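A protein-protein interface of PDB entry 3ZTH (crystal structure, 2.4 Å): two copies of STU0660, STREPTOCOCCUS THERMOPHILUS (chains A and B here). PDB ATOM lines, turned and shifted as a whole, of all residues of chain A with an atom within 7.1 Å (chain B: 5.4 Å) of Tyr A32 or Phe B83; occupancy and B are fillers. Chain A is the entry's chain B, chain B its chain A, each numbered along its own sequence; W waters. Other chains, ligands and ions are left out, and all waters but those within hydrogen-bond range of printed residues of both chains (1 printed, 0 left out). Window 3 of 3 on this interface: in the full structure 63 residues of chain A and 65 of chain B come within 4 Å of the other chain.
ND2 of Asn A28 lies within hydrogen-bond range of O of Ile B210 (2.7 Å).
NZ of Lys B180 lies close to OD1 of Asn B177 (3.3 Å).
ND2 of Asn A205 lies close to NZ of Lys A204 (3.4 Å).
The side-chain amide oxygen (OD1) of Asn A27 sits close to the side-chain carboxylate (OE1) of Glu A29, at 3.4 Å.
The side-chain amide nitrogen (ND2) of Asn B177 sits at hydrogen-bond distance from the backbone carbonyl oxygen (O) of Phe B209, 2.8 Å away.
The backbone carbonyl oxygen (O) of Glu B173 lies within hydrogen-bond range of the side-chain amino group (NZ) of Lys B180.
Asn A28 touches Phe B209 (CB to C, 3.6 Å).
N of Glu A29 touches O of Phe B209, 3.9 Å away.
OH of Tyr A32 touches CD2 of Phe B83, 3.5 Å away.
Tyr A32 touches Asn B177 (CD2 to ND2, 3.5 Å).
CD1 of Tyr A32 touches CD1 of Phe B209, 3.6 Å away.
Gln A36 touches Glu B173.
CE of Lys A204 touches CE1 of Phe B209, at 3.7 Å.
Asn A205 touches Phe B209.
Lys A31 touches none of the printed residues of chain B.
Tyr A32 touches just these residues of chain B: Phe B83 (3.5 Å), Asn B177 (3.5 Å) and Phe B209 (3.6 Å).
Of chain A, only Tyr A32 (3.5 Å) comes within 4 Å of Phe B83.
Printed residues of chain A within 4 Å of Glu B173: Gln A36 (3.7 Å).
Of the printed residues of chain A, Asn B177 touches Tyr A32.
Leu B181 touches none of the printed residues of chain A.
The nearest residue of chain A that does not touch Phe B83 is Gln A36 (6.8 Å).
The nearest printed residue of chain B that does not touch Glu A29 is Ile B210 (4.4 Å).
Of the 16 printed residues of chain B, 5 touch a printed residue of chain A.
Printed residues of chain B that touch a printed residue of chain A: Phe B83, Glu B173, Asn B177, Phe B209 and Ile B210.
Of the 16 printed residues of chain A, 6 touch a printed residue of chain B.
Printed residues of chain A that touch a printed residue of chain B: Asn A28, Glu A29, Tyr A32, Gln A36, Lys A204 and Asn A205.
No position is printed for both chains.
Water W1 lies within hydrogen-bond range of N of Phe B83 and OH of Tyr A32.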
ATOM      1  N   ASN A  27      34.604 -10.789 -25.391  1.00  0.00           N
ATOM      2  CA  ASN A  27      34.546 -10.645 -23.946  1.00  0.00           C
ATOM      3  C   ASN A  27      33.701  -9.412 -23.617  1.00  0.00           C
ATOM      4  O   ASN A  27      34.229  -8.365 -23.234  1.00  0.00           O
ATOM      5  CB  ASN A  27      35.944 -10.469 -23.369  1.00  0.00           C
ATOM      6  CG  ASN A  27      35.998 -10.764 -21.886  1.00  0.00           C
ATOM      7  OD1 ASN A  27      35.013 -10.591 -21.160  1.00  0.00           O
ATOM      8  ND2 ASN A  27      37.154 -11.202 -21.426  1.00  0.00           N
ATOM      9  N   ASN A  28      32.386  -9.544 -23.764  1.00  0.00           N
ATOM     10  CA  ASN A  28      31.473  -8.436 -23.504  1.00  0.00           C
ATOM     11  C   ASN A  28      31.592  -7.798 -22.114  1.00  0.00           C
ATOM     12  O   ASN A  28      31.457  -6.584 -21.964  1.00  0.00           O
ATOM     13  CB  ASN A  28      30.027  -8.891 -23.733  1.00  0.00           C
ATOM     14  CG  ASN A  28      29.700  -9.117 -25.213  1.00  0.00           C
ATOM     15  OD1 ASN A  28      30.557  -8.981 -26.095  1.00  0.00           O
ATOM     16  ND2 ASN A  28      28.449  -9.462 -25.485  1.00  0.00           N
ATOM     17  N   GLU A  29      31.850  -8.617 -21.102  1.00  0.00           N
ATOM     18  CA  GLU A  29      31.959  -8.125 -19.740  1.00  0.00           C
ATOM     19  C   GLU A  29      33.207  -7.279 -19.566  1.00  0.00           C
ATOM     20  O   GLU A  29      33.159  -6.209 -18.955  1.00  0.00           O
ATOM     21  CB  GLU A  29      31.967  -9.296 -18.753  1.00  0.00           C
ATOM     22  CG  GLU A  29      30.819 -10.272 -18.975  1.00  0.00           C
ATOM     23  CD  GLU A  29      31.157 -11.398 -19.962  1.00  0.00           C
ATOM     24  OE1 GLU A  29      31.641 -11.117 -21.088  1.00  0.00           O
ATOM     25  OE2 GLU A  29      30.926 -12.577 -19.603  1.00  0.00           O
ATOM     26  N   LEU A  30      34.323  -7.754 -20.105  1.00  0.00           N
ATOM     27  CA  LEU A  30      35.570  -7.008 -20.006  1.00  0.00           C
ATOM     28  C   LEU A  30      35.410  -5.682 -20.742  1.00  0.00           C
ATOM     29  O   LEU A  30      35.849  -4.636 -20.264  1.00  0.00           O
ATOM     30  CB  LEU A  30      36.722  -7.801 -20.618  1.00  0.00           C
ATOM     31  CG  LEU A  30      38.058  -7.061 -20.600  1.00  0.00           C
ATOM     32  CD1 LEU A  30      38.474  -6.772 -19.159  1.00  0.00           C
ATOM     33  CD2 LEU A  30      39.103  -7.906 -21.303  1.00  0.00           C
ATOM     34  N   LYS A  31      34.770  -5.727 -21.905  1.00  0.00           N
ATOM     35  CA  LYS A  31      34.553  -4.520 -22.682  1.00  0.00           C
ATOM     36  C   LYS A  31      33.685  -3.575 -21.875  1.00  0.00           C
ATOM     37  O   LYS A  31      33.943  -2.368 -21.831  1.00  0.00           O
ATOM     38  CB  LYS A  31      33.869  -4.848 -24.017  1.00  0.00           C
ATOM     39  CG  LYS A  31      34.839  -5.147 -25.146  1.00  0.00           C
ATOM     40  CD  LYS A  31      34.239  -6.075 -26.198  1.00  0.00           C
ATOM     41  CE  LYS A  31      32.954  -5.540 -26.792  1.00  0.00           C
ATOM     42  NZ  LYS A  31      32.427  -6.450 -27.846  1.00  0.00           N
ATOM     43  N   TYR A  32      32.666  -4.125 -21.219  1.00  0.00           N
ATOM     44  CA  TYR A  32      31.773  -3.289 -20.433  1.00  0.00           C
ATOM     45  C   TYR A  32      32.531  -2.645 -19.289  1.00  0.00           C
ATOM     46  O   TYR A  32      32.329  -1.472 -18.979  1.00  0.00           O
ATOM     47  CB  TYR A  32      30.608  -4.096 -19.869  1.00  0.00           C
ATOM     48  CG  TYR A  32      29.517  -3.213 -19.319  1.00  0.00           C
ATOM     49  CD1 TYR A  32      28.634  -2.556 -20.171  1.00  0.00           C
ATOM     50  CD2 TYR A  32      29.395  -2.999 -17.949  1.00  0.00           C
ATOM     51  CE1 TYR A  32      27.652  -1.702 -19.669  1.00  0.00           C
ATOM     52  CE2 TYR A  32      28.426  -2.150 -17.433  1.00  0.00           C
ATOM     53  CZ  TYR A  32      27.554  -1.501 -18.294  1.00  0.00           C
ATOM     54  OH  TYR A  32      26.596  -0.639 -17.779  1.00  0.00           O
ATOM     55  N   TYR A  33      33.406  -3.419 -18.660  1.00  0.00           N
ATOM     56  CA  TYR A  33      34.195  -2.902 -17.557  1.00  0.00           C
ATOM     57  C   TYR A  33      35.039  -1.733 -18.072  1.00  0.00           C
ATOM     58  O   TYR A  33      35.023  -0.636 -17.511  1.00  0.00           O
ATOM     59  CB  TYR A  33      35.106  -4.000 -16.999  1.00  0.00           C
ATOM     60  CG  TYR A  33      36.097  -3.498 -15.975  1.00  0.00           C
ATOM     61  CD1 TYR A  33      35.690  -3.156 -14.687  1.00  0.00           C
ATOM     62  CD2 TYR A  33      37.437  -3.307 -16.316  1.00  0.00           C
ATOM     63  CE1 TYR A  33      36.594  -2.629 -13.766  1.00  0.00           C
ATOM     64  CE2 TYR A  33      38.349  -2.781 -15.403  1.00  0.00           C
ATOM     65  CZ  TYR A  33      37.920  -2.442 -14.137  1.00  0.00           C
ATOM     66  OH  TYR A  33      38.811  -1.892 -13.247  1.00  0.00           O
ATOM     67  N   THR A  34      35.765  -1.977 -19.156  1.00  0.00           N
ATOM     68  CA  THR A  34      36.624  -0.963 -19.737  1.00  0.00           C
ATOM     69  C   THR A  34      35.885   0.338 -20.024  1.00  0.00           C
ATOM     70  O   THR A  34      36.402   1.425 -19.767  1.00  0.00           O
ATOM     71  CB  THR A  34      37.276  -1.489 -21.020  1.00  0.00           C
ATOM     72  OG1 THR A  34      38.061  -2.646 -20.699  1.00  0.00           O
ATOM     73  CG2 THR A  34      38.173  -0.430 -21.640  1.00  0.00           C
ATOM     74  N   TRP A  35      34.676   0.238 -20.549  1.00  0.00           N
ATOM     75  CA  TRP A  35      33.894   1.430 -20.834  1.00  0.00           C
ATOM     76  C   TRP A  35      33.515   2.154 -19.537  1.00  0.00           C
ATOM     77  O   TRP A  35      33.519   3.379 -19.470  1.00  0.00           O
ATOM     78  CB  TRP A  35      32.615   1.055 -21.591  1.00  0.00           C
ATOM     79  CG  TRP A  35      31.606   2.138 -21.545  1.00  0.00           C
ATOM     80  CD1 TRP A  35      31.608   3.289 -22.272  1.00  0.00           C
ATOM     81  CD2 TRP A  35      30.504   2.235 -20.640  1.00  0.00           C
ATOM     82  NE1 TRP A  35      30.579   4.103 -21.874  1.00  0.00           N
ATOM     83  CE2 TRP A  35      29.886   3.484 -20.870  1.00  0.00           C
ATOM     84  CE3 TRP A  35      29.981   1.391 -19.649  1.00  0.00           C
ATOM     85  CZ2 TRP A  35      28.764   3.917 -20.141  1.00  0.00           C
ATOM     86  CZ3 TRP A  35      28.864   1.821 -18.921  1.00  0.00           C
ATOM     87  CH2 TRP A  35      28.270   3.073 -19.172  1.00  0.00           C
ATOM     88  N   GLN A  36      33.179   1.378 -18.513  1.00  0.00           N
ATOM     89  CA  GLN A  36      32.774   1.917 -17.222  1.00  0.00           C
ATOM     90  C   GLN A  36      33.902   2.725 -16.583  1.00  0.00           C
ATOM     91  O   GLN A  36      33.694   3.864 -16.145  1.00  0.00           O
ATOM     92  CB  GLN A  36      32.363   0.766 -16.306  1.00  0.00           C
ATOM     93  CG  GLN A  36      31.634   1.170 -15.037  1.00  0.00           C
ATOM     94  CD  GLN A  36      30.250   1.743 -15.301  1.00  0.00           C
ATOM     95  OE1 GLN A  36      30.103   2.934 -15.592  1.00  0.00           O
ATOM     96  NE2 GLN A  36      29.227   0.892 -15.209  1.00  0.00           N
ATOM     97  N   ILE A  37      35.091   2.131 -16.521  1.00  0.00           N
ATOM     98  CA  ILE A  37      36.255   2.802 -15.948  1.00  0.00           C
ATOM     99  C   ILE A  37      36.563   4.073 -16.739  1.00  0.00           C
ATOM    100  O   ILE A  37      36.779   5.133 -16.163  1.00  0.00           O
ATOM    101  CB  ILE A  37      37.500   1.873 -15.968  1.00  0.00           C
ATOM    102  CG1 ILE A  37      37.335   0.763 -14.934  1.00  0.00           C
ATOM    103  CG2 ILE A  37      38.759   2.661 -15.662  1.00  0.00           C
ATOM    104  CD1 ILE A  37      37.344   1.255 -13.501  1.00  0.00           C
ATOM    105  N   LEU A  38      36.577   3.954 -18.064  1.00  0.00           N
ATOM    106  CA  LEU A  38      36.850   5.089 -18.944  1.00  0.00           C
ATOM    107  C   LEU A  38      35.925   6.263 -18.664  1.00  0.00           C
ATOM    108  O   LEU A  38      36.377   7.397 -18.572  1.00  0.00           O
ATOM    109  CB  LEU A  38      36.701   4.685 -20.423  1.00  0.00           C
ATOM    110  CG  LEU A  38      37.808   3.843 -21.061  1.00  0.00           C
ATOM    111  CD1 LEU A  38      37.432   3.476 -22.487  1.00  0.00           C
ATOM    112  CD2 LEU A  38      39.109   4.625 -21.042  1.00  0.00           C
ATOM    113  N   LYS A 204      28.786   4.052 -27.990  1.00  0.00           N
ATOM    114  CA  LYS A 204      28.442   2.666 -27.698  1.00  0.00           C
ATOM    115  C   LYS A 204      26.941   2.501 -27.930  1.00  0.00           C
ATOM    116  O   LYS A 204      26.190   3.461 -27.783  1.00  0.00           O
ATOM    117  CB  LYS A 204      28.806   2.367 -26.235  1.00  0.00           C
ATOM    118  CG  LYS A 204      28.687   0.914 -25.810  1.00  0.00           C
ATOM    119  CD  LYS A 204      29.387   0.652 -24.466  1.00  0.00           C
ATOM    120  CE  LYS A 204      28.404   0.511 -23.287  1.00  0.00           C
ATOM    121  NZ  LYS A 204      27.666   1.769 -22.925  1.00  0.00           N
ATOM    122  N   ASN A 205      26.513   1.300 -28.321  1.00  0.00           N
ATOM    123  CA  ASN A 205      25.095   0.991 -28.554  1.00  0.00           C
ATOM    124  C   ASN A 205      24.405   1.632 -29.755  1.00  0.00           C
ATOM    125  O   ASN A 205      23.238   1.359 -29.991  1.00  0.00           O
ATOM    126  CB  ASN A 205      24.257   1.335 -27.317  1.00  0.00           C
ATOM    127  CG  ASN A 205      24.825   0.750 -26.047  1.00  0.00           C
ATOM    128  OD1 ASN A 205      25.055  -0.456 -25.953  1.00  0.00           O
ATOM    129  ND2 ASN A 205      25.057   1.606 -25.055  1.00  0.00           N
ATOM    130  N   PHE A 237      32.744   1.265 -29.800  1.00  0.00           N
ATOM    131  CA  PHE A 237      32.556  -0.105 -29.335  1.00  0.00           C
ATOM    132  C   PHE A 237      31.594  -0.754 -30.336  1.00  0.00           C
ATOM    133  O   PHE A 237      30.404  -0.912 -30.057  1.00  0.00           O
ATOM    134  CB  PHE A 237      31.923  -0.107 -27.948  1.00  0.00           C
ATOM    135  CG  PHE A 237      32.852   0.305 -26.848  1.00  0.00           C
ATOM    136  CD1 PHE A 237      33.065   1.649 -26.567  1.00  0.00           C
ATOM    137  CD2 PHE A 237      33.480  -0.651 -26.057  1.00  0.00           C
ATOM    138  CE1 PHE A 237      33.886   2.037 -25.508  1.00  0.00           C
ATOM    139  CE2 PHE A 237      34.303  -0.277 -24.993  1.00  0.00           C
ATOM    140  CZ  PHE A 237      34.505   1.071 -24.717  1.00  0.00           C
ATOM    141  N   LEU A 257      39.195  -7.469 -27.435  1.00  0.00           N
ATOM    142  CA  LEU A 257      39.123  -7.904 -26.043  1.00  0.00           C
ATOM    143  C   LEU A 257      38.271  -9.166 -25.962  1.00  0.00           C
ATOM    144  O   LEU A 257      37.040  -9.099 -25.932  1.00  0.00           O
ATOM    145  CB  LEU A 257      38.512  -6.820 -25.143  1.00  0.00           C
ATOM    146  CG  LEU A 257      39.004  -5.365 -25.198  1.00  0.00           C
ATOM    147  CD1 LEU A 257      38.595  -4.665 -23.900  1.00  0.00           C
ATOM    148  CD2 LEU A 257      40.510  -5.298 -25.392  1.00  0.00           C
ATOM    149  N   SER B  81      16.492  -0.779 -20.996  1.00  0.00           N
ATOM    150  CA  SER B  81      17.339  -0.537 -22.155  1.00  0.00           C
ATOM    151  C   SER B  81      18.763  -0.234 -21.735  1.00  0.00           C
ATOM    152  O   SER B  81      19.600   0.097 -22.568  1.00  0.00           O
ATOM    153  CB  SER B  81      16.779   0.612 -22.996  1.00  0.00           C
ATOM    154  OG  SER B  81      15.585   0.204 -23.652  1.00  0.00           O
ATOM    155  N   SER B  82      19.029  -0.352 -20.439  1.00  0.00           N
ATOM    156  CA  SER B  82      20.365  -0.128 -19.894  1.00  0.00           C
ATOM    157  C   SER B  82      20.411  -0.681 -18.480  1.00  0.00           C
ATOM    158  O   SER B  82      19.367  -0.872 -17.848  1.00  0.00           O
ATOM    159  CB  SER B  82      20.690   1.361 -19.835  1.00  0.00           C
ATOM    160  OG  SER B  82      20.014   1.969 -18.746  1.00  0.00           O
ATOM    161  N   PHE B  83      21.612  -0.940 -17.975  1.00  0.00           N
ATOM    162  CA  PHE B  83      21.709  -1.434 -16.613  1.00  0.00           C
ATOM    163  C   PHE B  83      21.267  -0.352 -15.619  1.00  0.00           C
ATOM    164  O   PHE B  83      20.888  -0.650 -14.480  1.00  0.00           O
ATOM    165  CB  PHE B  83      23.127  -1.905 -16.309  1.00  0.00           C
ATOM    166  CG  PHE B  83      23.440  -3.259 -16.869  1.00  0.00           C
ATOM    167  CD1 PHE B  83      22.595  -4.339 -16.614  1.00  0.00           C
ATOM    168  CD2 PHE B  83      24.565  -3.462 -17.652  1.00  0.00           C
ATOM    169  CE1 PHE B  83      22.869  -5.600 -17.134  1.00  0.00           C
ATOM    170  CE2 PHE B  83      24.847  -4.724 -18.177  1.00  0.00           C
ATOM    171  CZ  PHE B  83      23.997  -5.793 -17.918  1.00  0.00           C
ATOM    172  N   LYS B  84      21.291   0.905 -16.051  1.00  0.00           N
ATOM    173  CA  LYS B  84      20.873   1.980 -15.168  1.00  0.00           C
ATOM    174  C   LYS B  84      19.377   1.846 -14.907  1.00  0.00           C
ATOM    175  O   LYS B  84      18.911   2.112 -13.799  1.00  0.00           O
ATOM    176  CB  LYS B  84      21.174   3.346 -15.782  1.00  0.00           C
ATOM    177  CG  LYS B  84      20.730   4.510 -14.903  1.00  0.00           C
ATOM    178  CD  LYS B  84      20.807   5.838 -15.641  1.00  0.00           C
ATOM    179  CE  LYS B  84      20.214   6.974 -14.808  1.00  0.00           C
ATOM    180  NZ  LYS B  84      20.189   8.273 -15.555  1.00  0.00           N
ATOM    181  N   ASP B  85      18.624   1.433 -15.924  1.00  0.00           N
ATOM    182  CA  ASP B  85      17.185   1.260 -15.752  1.00  0.00           C
ATOM    183  C   ASP B  85      16.934   0.135 -14.755  1.00  0.00           C
ATOM    184  O   ASP B  85      15.980   0.171 -13.971  1.00  0.00           O
ATOM    185  CB  ASP B  85      16.502   0.904 -17.075  1.00  0.00           C
ATOM    186  CG  ASP B  85      16.573   2.017 -18.083  1.00  0.00           C
ATOM    187  OD1 ASP B  85      16.603   3.191 -17.659  1.00  0.00           O
ATOM    188  OD2 ASP B  85      16.579   1.720 -19.296  1.00  0.00           O
ATOM    189  N   LEU B  86      17.801  -0.869 -14.798  1.00  0.00           N
ATOM    190  CA  LEU B  86      17.685  -2.001 -13.907  1.00  0.00           C
ATOM    191  C   LEU B  86      17.923  -1.559 -12.454  1.00  0.00           C
ATOM    192  O   LEU B  86      17.140  -1.897 -11.556  1.00  0.00           O
ATOM    193  CB  LEU B  86      18.666  -3.084 -14.339  1.00  0.00           C
ATOM    194  CG  LEU B  86      18.399  -4.470 -13.750  1.00  0.00           C
ATOM    195  CD1 LEU B  86      18.883  -5.535 -14.728  1.00  0.00           C
ATOM    196  CD2 LEU B  86      19.075  -4.596 -12.386  1.00  0.00           C
ATOM    197  N   LEU B  87      18.987  -0.798 -12.218  1.00  0.00           N
ATOM    198  CA  LEU B  87      19.254  -0.314 -10.869  1.00  0.00           C
ATOM    199  C   LEU B  87      18.064   0.511 -10.375  1.00  0.00           C
ATOM    200  O   LEU B  87      17.648   0.391  -9.220  1.00  0.00           O
ATOM    201  CB  LEU B  87      20.514   0.548 -10.844  1.00  0.00           C
ATOM    202  CG  LEU B  87      20.830   1.237  -9.507  1.00  0.00           C
ATOM    203  CD1 LEU B  87      21.002   0.196  -8.408  1.00  0.00           C
ATOM    204  CD2 LEU B  87      22.085   2.075  -9.651  1.00  0.00           C
ATOM    205  N   GLU B  88      17.513   1.341 -11.260  1.00  0.00           N
ATOM    206  CA  GLU B  88      16.371   2.190 -10.916  1.00  0.00           C
ATOM    207  C   GLU B  88      15.134   1.399 -10.508  1.00  0.00           C
ATOM    208  O   GLU B  88      14.358   1.850  -9.663  1.00  0.00           O
ATOM    209  CB  GLU B  88      16.036   3.128 -12.079  1.00  0.00           C
ATOM    210  CG  GLU B  88      16.696   4.497 -11.953  1.00  0.00           C
ATOM    211  CD  GLU B  88      16.654   5.316 -13.241  1.00  0.00           C
ATOM    212  OE1 GLU B  88      15.591   5.339 -13.911  1.00  0.00           O
ATOM    213  OE2 GLU B  88      17.688   5.948 -13.571  1.00  0.00           O
ATOM    214  N   PHE B 172      26.639  -1.167  -7.335  1.00  0.00           N
ATOM    215  CA  PHE B 172      25.865  -1.947  -8.287  1.00  0.00           C
ATOM    216  C   PHE B 172      26.574  -2.124  -9.627  1.00  0.00           C
ATOM    217  O   PHE B 172      26.503  -3.180 -10.245  1.00  0.00           O
ATOM    218  CB  PHE B 172      24.525  -1.262  -8.519  1.00  0.00           C
ATOM    219  CG  PHE B 172      23.686  -1.931  -9.547  1.00  0.00           C
ATOM    220  CD1 PHE B 172      23.143  -3.186  -9.307  1.00  0.00           C
ATOM    221  CD2 PHE B 172      23.428  -1.306 -10.761  1.00  0.00           C
ATOM    222  CE1 PHE B 172      22.349  -3.810 -10.262  1.00  0.00           C
ATOM    223  CE2 PHE B 172      22.635  -1.921 -11.723  1.00  0.00           C
ATOM    224  CZ  PHE B 172      22.094  -3.176 -11.472  1.00  0.00           C
ATOM    225  N   GLU B 173      27.251  -1.075 -10.070  1.00  0.00           N
ATOM    226  CA  GLU B 173      27.961  -1.093 -11.338  1.00  0.00           C
ATOM    227  C   GLU B 173      29.011  -2.185 -11.423  1.00  0.00           C
ATOM    228  O   GLU B 173      29.211  -2.782 -12.479  1.00  0.00           O
ATOM    229  CB  GLU B 173      28.618   0.267 -11.594  1.00  0.00           C
ATOM    230  CG  GLU B 173      27.625   1.421 -11.707  1.00  0.00           C
ATOM    231  CD  GLU B 173      27.223   2.024 -10.364  1.00  0.00           C
ATOM    232  OE1 GLU B 173      26.914   1.273  -9.415  1.00  0.00           O
ATOM    233  OE2 GLU B 173      27.204   3.264 -10.259  1.00  0.00           O
ATOM    234  N   ASN B 177      27.493  -8.282 -14.608  1.00  0.00           N
ATOM    235  CA  ASN B 177      26.311  -8.025 -15.423  1.00  0.00           C
ATOM    236  C   ASN B 177      25.252  -9.121 -15.334  1.00  0.00           C
ATOM    237  O   ASN B 177      24.070  -8.820 -15.171  1.00  0.00           O
ATOM    238  CB  ASN B 177      26.710  -7.770 -16.883  1.00  0.00           C
ATOM    239  CG  ASN B 177      27.357  -6.405 -17.077  1.00  0.00           C
ATOM    240  OD1 ASN B 177      27.410  -5.605 -16.149  1.00  0.00           O
ATOM    241  ND2 ASN B 177      27.841  -6.132 -18.279  1.00  0.00           N
ATOM    242  N   LYS B 180      23.453  -8.800 -12.207  1.00  0.00           N
ATOM    243  CA  LYS B 180      22.533  -7.669 -12.219  1.00  0.00           C
ATOM    244  C   LYS B 180      21.162  -8.137 -12.700  1.00  0.00           C
ATOM    245  O   LYS B 180      20.125  -7.837 -12.089  1.00  0.00           O
ATOM    246  CB  LYS B 180      23.037  -6.568 -13.152  1.00  0.00           C
ATOM    247  CG  LYS B 180      24.109  -5.666 -12.572  1.00  0.00           C
ATOM    248  CD  LYS B 180      24.300  -4.452 -13.485  1.00  0.00           C
ATOM    249  CE  LYS B 180      25.624  -4.465 -14.237  1.00  0.00           C
ATOM    250  NZ  LYS B 180      26.744  -3.933 -13.421  1.00  0.00           N
ATOM    251  N   LEU B 181      21.171  -8.892 -13.789  1.00  0.00           N
ATOM    252  CA  LEU B 181      19.941  -9.402 -14.371  1.00  0.00           C
ATOM    253  C   LEU B 181      19.284 -10.419 -13.441  1.00  0.00           C
ATOM    254  O   LEU B 181      18.067 -10.377 -13.218  1.00  0.00           O
ATOM    255  CB  LEU B 181      20.248 -10.030 -15.735  1.00  0.00           C
ATOM    256  CG  LEU B 181      20.782  -9.062 -16.807  1.00  0.00           C
ATOM    257  CD1 LEU B 181      21.327  -9.848 -17.980  1.00  0.00           C
ATOM    258  CD2 LEU B 181      19.675  -8.105 -17.258  1.00  0.00           C
ATOM    259  N   ILE B 206      21.127  -5.222 -24.009  1.00  0.00           N
ATOM    260  CA  ILE B 206      21.842  -6.055 -23.052  1.00  0.00           C
ATOM    261  C   ILE B 206      22.774  -7.096 -23.673  1.00  0.00           C
ATOM    262  O   ILE B 206      23.825  -7.404 -23.105  1.00  0.00           O
ATOM    263  CB  ILE B 206      20.848  -6.752 -22.107  1.00  0.00           C
ATOM    264  CG1 ILE B 206      20.084  -5.691 -21.320  1.00  0.00           C
ATOM    265  CG2 ILE B 206      21.579  -7.680 -21.152  1.00  0.00           C
ATOM    266  CD1 ILE B 206      20.993  -4.642 -20.679  1.00  0.00           C
ATOM    267  N   PHE B 209      26.391  -6.508 -23.538  1.00  0.00           N
ATOM    268  CA  PHE B 209      27.064  -6.444 -22.247  1.00  0.00           C
ATOM    269  C   PHE B 209      27.396  -7.771 -21.572  1.00  0.00           C
ATOM    270  O   PHE B 209      28.061  -7.787 -20.543  1.00  0.00           O
ATOM    271  CB  PHE B 209      26.255  -5.566 -21.292  1.00  0.00           C
ATOM    272  CG  PHE B 209      25.814  -4.259 -21.898  1.00  0.00           C
ATOM    273  CD1 PHE B 209      26.564  -3.654 -22.912  1.00  0.00           C
ATOM    274  CD2 PHE B 209      24.662  -3.614 -21.435  1.00  0.00           C
ATOM    275  CE1 PHE B 209      26.177  -2.424 -23.454  1.00  0.00           C
ATOM    276  CE2 PHE B 209      24.262  -2.383 -21.967  1.00  0.00           C
ATOM    277  CZ  PHE B 209      25.021  -1.785 -22.980  1.00  0.00           C
ATOM    278  N   ILE B 210      26.941  -8.882 -22.136  1.00  0.00           N
ATOM    279  CA  ILE B 210      27.256 -10.178 -21.554  1.00  0.00           C
ATOM    280  C   ILE B 210      27.567 -11.186 -22.639  1.00  0.00           C
ATOM    281  O   ILE B 210      27.123 -11.039 -23.775  1.00  0.00           O
ATOM    282  CB  ILE B 210      26.108 -10.720 -20.674  1.00  0.00           C
ATOM    283  CG1 ILE B 210      24.839 -10.908 -21.499  1.00  0.00           C
ATOM    284  CG2 ILE B 210      25.832  -9.751 -19.533  1.00  0.00           C
ATOM    285  CD1 ILE B 210      23.697 -11.469 -20.679  1.00  0.00           C
HETATM  286  O   HOH W   1      24.086   0.044 -19.438  1.00  0.00           O
